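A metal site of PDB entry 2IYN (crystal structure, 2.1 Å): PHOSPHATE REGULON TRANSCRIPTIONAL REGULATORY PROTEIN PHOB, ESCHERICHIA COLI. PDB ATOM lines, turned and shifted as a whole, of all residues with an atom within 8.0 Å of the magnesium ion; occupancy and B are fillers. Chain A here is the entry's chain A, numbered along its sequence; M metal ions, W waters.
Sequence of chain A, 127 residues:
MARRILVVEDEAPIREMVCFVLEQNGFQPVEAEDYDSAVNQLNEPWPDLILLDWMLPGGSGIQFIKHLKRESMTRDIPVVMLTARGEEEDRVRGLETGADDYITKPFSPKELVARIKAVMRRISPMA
NZ of Lys 105 lies within salt-bridge range of OD2 of Asp 53, 2.7 Å away. The backbone NH of Asp 53 is in hydrogen-bond range of the backbone carbonyl oxygen of Val 8.
The magnesium ion is bound by OD1 of Asp 53 (2.0 Å), water W1 (2.0 Å), OD1 of Asp 10 (2.0 Å), water W2 (2.1 Å) and O of Met 55 (2.5 Å).
Three residues have an atom within 4 Å of the magnesium ion: Asp 10, Asp 53 and Met 55.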
ATOM      1  N   VAL A   8     -23.132  16.767 -30.779  1.00  0.00           N
ATOM      2  CA  VAL A   8     -24.573  16.684 -31.096  1.00  0.00           C
ATOM      3  C   VAL A   8     -25.353  16.866 -29.801  1.00  0.00           C
ATOM      4  O   VAL A   8     -25.373  15.990 -28.948  1.00  0.00           O
ATOM      5  CB  VAL A   8     -24.928  15.330 -31.767  1.00  0.00           C
ATOM      6  CG1 VAL A   8     -26.408  15.234 -32.152  1.00  0.00           C
ATOM      7  CG2 VAL A   8     -24.078  15.074 -32.972  1.00  0.00           C
ATOM      8  N   GLU A   9     -26.023  18.014 -29.668  1.00  0.00           N
ATOM      9  CA  GLU A   9     -26.571  18.442 -28.390  1.00  0.00           C
ATOM     10  C   GLU A   9     -27.488  19.646 -28.566  1.00  0.00           C
ATOM     11  O   GLU A   9     -27.082  20.706 -29.081  1.00  0.00           O
ATOM     12  CB  GLU A   9     -25.403  18.774 -27.429  1.00  0.00           C
ATOM     13  CG  GLU A   9     -25.816  19.567 -26.201  1.00  0.00           C
ATOM     14  CD  GLU A   9     -26.700  18.771 -25.249  1.00  0.00           C
ATOM     15  OE1 GLU A   9     -26.240  17.761 -24.682  1.00  0.00           O
ATOM     16  OE2 GLU A   9     -27.871  19.143 -25.083  1.00  0.00           O
ATOM     17  N   ASP A  10     -28.741  19.505 -28.122  1.00  0.00           N
ATOM     18  CA  ASP A  10     -29.760  20.475 -28.466  1.00  0.00           C
ATOM     19  C   ASP A  10     -29.875  21.633 -27.510  1.00  0.00           C
ATOM     20  O   ASP A  10     -30.454  22.675 -27.856  1.00  0.00           O
ATOM     21  CB  ASP A  10     -31.114  19.770 -28.590  1.00  0.00           C
ATOM     22  CG  ASP A  10     -31.467  18.979 -27.353  1.00  0.00           C
ATOM     23  OD1 ASP A  10     -30.656  18.121 -26.937  1.00  0.00           O
ATOM     24  OD2 ASP A  10     -32.546  19.110 -26.749  1.00  0.00           O
ATOM     25  N   GLU A  11     -29.373  21.459 -26.282  1.00  0.00           N
ATOM     26  CA  GLU A  11     -29.337  22.555 -25.329  1.00  0.00           C
ATOM     27  C   GLU A  11     -28.088  23.346 -25.584  1.00  0.00           C
ATOM     28  O   GLU A  11     -26.951  22.912 -25.266  1.00  0.00           O
ATOM     29  CB  GLU A  11     -29.369  22.031 -23.893  1.00  0.00           C
ATOM     30  CG  GLU A  11     -30.693  21.402 -23.513  1.00  0.00           C
ATOM     31  CD  GLU A  11     -30.627  20.771 -22.146  1.00  0.00           C
ATOM     32  OE1 GLU A  11     -30.381  19.554 -22.035  1.00  0.00           O
ATOM     33  OE2 GLU A  11     -30.803  21.513 -21.188  1.00  0.00           O
ATOM     34  N   ILE A  14     -25.128  23.906 -22.904  1.00  0.00           N
ATOM     35  CA  ILE A  14     -24.357  22.675 -22.796  1.00  0.00           C
ATOM     36  C   ILE A  14     -23.459  22.444 -24.025  1.00  0.00           C
ATOM     37  O   ILE A  14     -22.265  22.205 -23.889  1.00  0.00           O
ATOM     38  CB  ILE A  14     -25.298  21.465 -22.658  1.00  0.00           C
ATOM     39  CG1 ILE A  14     -26.190  21.616 -21.406  1.00  0.00           C
ATOM     40  CG2 ILE A  14     -24.491  20.219 -22.564  1.00  0.00           C
ATOM     41  CD1 ILE A  14     -26.866  20.295 -21.004  1.00  0.00           C
ATOM     42  N   GLU A  33     -27.266  21.065 -33.481  1.00  0.00           N
ATOM     43  CA  GLU A  33     -28.360  21.333 -32.540  1.00  0.00           C
ATOM     44  C   GLU A  33     -29.535  20.321 -32.524  1.00  0.00           C
ATOM     45  O   GLU A  33     -30.340  20.306 -31.607  1.00  0.00           O
ATOM     46  CB  GLU A  33     -28.871  22.795 -32.689  1.00  0.00           C
ATOM     47  CG  GLU A  33     -29.927  23.003 -33.782  1.00  0.00           C
ATOM     48  CD  GLU A  33     -30.288  24.481 -34.016  1.00  0.00           C
ATOM     49  OE1 GLU A  33     -31.081  24.764 -34.955  1.00  0.00           O
ATOM     50  OE2 GLU A  33     -29.795  25.367 -33.283  1.00  0.00           O
ATOM     51  N   LEU A  52     -22.594  12.502 -28.385  1.00  0.00           N
ATOM     52  CA  LEU A  52     -23.973  12.361 -28.824  1.00  0.00           C
ATOM     53  C   LEU A  52     -24.931  12.483 -27.675  1.00  0.00           C
ATOM     54  O   LEU A  52     -24.931  11.607 -26.801  1.00  0.00           O
ATOM     55  CB  LEU A  52     -24.183  11.006 -29.510  1.00  0.00           C
ATOM     56  CG  LEU A  52     -25.579  10.687 -30.039  1.00  0.00           C
ATOM     57  CD1 LEU A  52     -26.070  11.763 -31.033  1.00  0.00           C
ATOM     58  CD2 LEU A  52     -25.549   9.334 -30.732  1.00  0.00           C
ATOM     59  N   ASP A  53     -25.750  13.520 -27.675  1.00  0.00           N
ATOM     60  CA  ASP A  53     -26.780  13.682 -26.631  1.00  0.00           C
ATOM     61  C   ASP A  53     -27.847  12.597 -26.855  1.00  0.00           C
ATOM     62  O   ASP A  53     -28.134  12.203 -28.004  1.00  0.00           O
ATOM     63  CB  ASP A  53     -27.371  15.094 -26.680  1.00  0.00           C
ATOM     64  CG  ASP A  53     -28.554  15.278 -25.756  1.00  0.00           C
ATOM     65  OD1 ASP A  53     -29.505  15.978 -26.153  1.00  0.00           O
ATOM     66  OD2 ASP A  53     -28.629  14.811 -24.594  1.00  0.00           O
ATOM     67  N   TRP A  54     -28.439  12.115 -25.762  1.00  0.00           N
ATOM     68  CA  TRP A  54     -29.331  10.976 -25.790  1.00  0.00           C
ATOM     69  C   TRP A  54     -30.644  11.234 -26.521  1.00  0.00           C
ATOM     70  O   TRP A  54     -31.206  10.332 -27.127  1.00  0.00           O
ATOM     71  CB  TRP A  54     -29.529  10.462 -24.367  1.00  0.00           C
ATOM     72  CG  TRP A  54     -30.961  10.317 -23.944  1.00  0.00           C
ATOM     73  CD1 TRP A  54     -31.873   9.370 -24.399  1.00  0.00           C
ATOM     74  CD2 TRP A  54     -31.653  11.110 -22.979  1.00  0.00           C
ATOM     75  NE1 TRP A  54     -33.092   9.555 -23.774  1.00  0.00           N
ATOM     76  CE2 TRP A  54     -32.983  10.617 -22.896  1.00  0.00           C
ATOM     77  CE3 TRP A  54     -31.272  12.198 -22.154  1.00  0.00           C
ATOM     78  CZ2 TRP A  54     -33.944  11.160 -22.035  1.00  0.00           C
ATOM     79  CZ3 TRP A  54     -32.233  12.741 -21.292  1.00  0.00           C
ATOM     80  CH2 TRP A  54     -33.548  12.221 -21.241  1.00  0.00           C
ATOM     81  N   MET A  55     -31.139  12.482 -26.477  1.00  0.00           N
ATOM     82  CA  MET A  55     -32.393  12.839 -27.137  1.00  0.00           C
ATOM     83  C   MET A  55     -32.309  14.213 -27.845  1.00  0.00           C
ATOM     84  O   MET A  55     -31.836  15.177 -27.245  1.00  0.00           O
ATOM     85  CB  MET A  55     -33.526  12.894 -26.097  1.00  0.00           C
ATOM     86  CG  MET A  55     -34.937  12.944 -26.686  1.00  0.00           C
ATOM     87  SD  MET A  55     -35.275  11.662 -27.912  1.00  0.00           S
ATOM     88  CE  MET A  55     -35.292  10.056 -26.735  1.00  0.00           C
ATOM     89  N   LEU A  56     -32.817  14.314 -29.068  1.00  0.00           N
ATOM     90  CA  LEU A  56     -32.799  15.596 -29.794  1.00  0.00           C
ATOM     91  C   LEU A  56     -34.069  15.816 -30.535  1.00  0.00           C
ATOM     92  O   LEU A  56     -34.722  14.875 -30.898  1.00  0.00           O
ATOM     93  CB  LEU A  56     -31.660  15.635 -30.819  1.00  0.00           C
ATOM     94  CG  LEU A  56     -30.260  15.266 -30.327  1.00  0.00           C
ATOM     95  CD1 LEU A  56     -29.553  14.476 -31.438  1.00  0.00           C
ATOM     96  CD2 LEU A  56     -29.525  16.487 -29.959  1.00  0.00           C
ATOM     97  N   PRO A  57     -34.417  17.083 -30.774  1.00  0.00           N
ATOM     98  CA  PRO A  57     -35.523  17.413 -31.689  1.00  0.00           C
ATOM     99  C   PRO A  57     -35.331  16.686 -33.041  1.00  0.00           C
ATOM    100  O   PRO A  57     -34.258  16.792 -33.647  1.00  0.00           O
ATOM    101  CB  PRO A  57     -35.352  18.918 -31.876  1.00  0.00           C
ATOM    102  CG  PRO A  57     -34.720  19.385 -30.579  1.00  0.00           C
ATOM    103  CD  PRO A  57     -33.787  18.288 -30.207  1.00  0.00           C
ATOM    104  N   GLY A  59     -35.116  13.391 -33.469  1.00  0.00           N
ATOM    105  CA  GLY A  59     -34.598  12.022 -33.335  1.00  0.00           C
ATOM    106  C   GLY A  59     -33.762  11.753 -32.113  1.00  0.00           C
ATOM    107  O   GLY A  59     -33.123  12.655 -31.566  1.00  0.00           O
ATOM    108  N   LEU A  82     -23.774  11.195 -24.378  1.00  0.00           N
ATOM    109  CA  LEU A  82     -23.995  12.130 -23.263  1.00  0.00           C
ATOM    110  C   LEU A  82     -25.365  11.879 -22.707  1.00  0.00           C
ATOM    111  O   LEU A  82     -26.344  12.043 -23.414  1.00  0.00           O
ATOM    112  CB  LEU A  82     -24.025  13.578 -23.755  1.00  0.00           C
ATOM    113  CG  LEU A  82     -22.796  14.114 -24.459  1.00  0.00           C
ATOM    114  CD1 LEU A  82     -23.115  15.441 -25.168  1.00  0.00           C
ATOM    115  CD2 LEU A  82     -21.702  14.323 -23.443  1.00  0.00           C
ATOM    116  N   LYS A 105     -24.140  14.048 -17.651  1.00  0.00           N
ATOM    117  CA  LYS A 105     -24.320  15.501 -17.506  1.00  0.00           C
ATOM    118  C   LYS A 105     -24.929  15.839 -16.146  1.00  0.00           C
ATOM    119  O   LYS A 105     -25.969  15.270 -15.791  1.00  0.00           O
ATOM    120  CB  LYS A 105     -25.245  16.056 -18.610  1.00  0.00           C
ATOM    121  CG  LYS A 105     -24.803  15.772 -20.011  1.00  0.00           C
ATOM    122  CD  LYS A 105     -25.627  16.501 -21.089  1.00  0.00           C
ATOM    123  CE  LYS A 105     -26.782  15.660 -21.620  1.00  0.00           C
ATOM    124  NZ  LYS A 105     -27.671  16.402 -22.602  1.00  0.00           N
HETATM  125 MG    MG M   1     -31.188  16.831 -25.459  1.00  0.00          MG
HETATM  126  O   HOH W   1     -31.271  15.289 -24.167  1.00  0.00           O
HETATM  127  O   HOH W   2     -29.702  17.567 -24.126  1.00  0.00           O
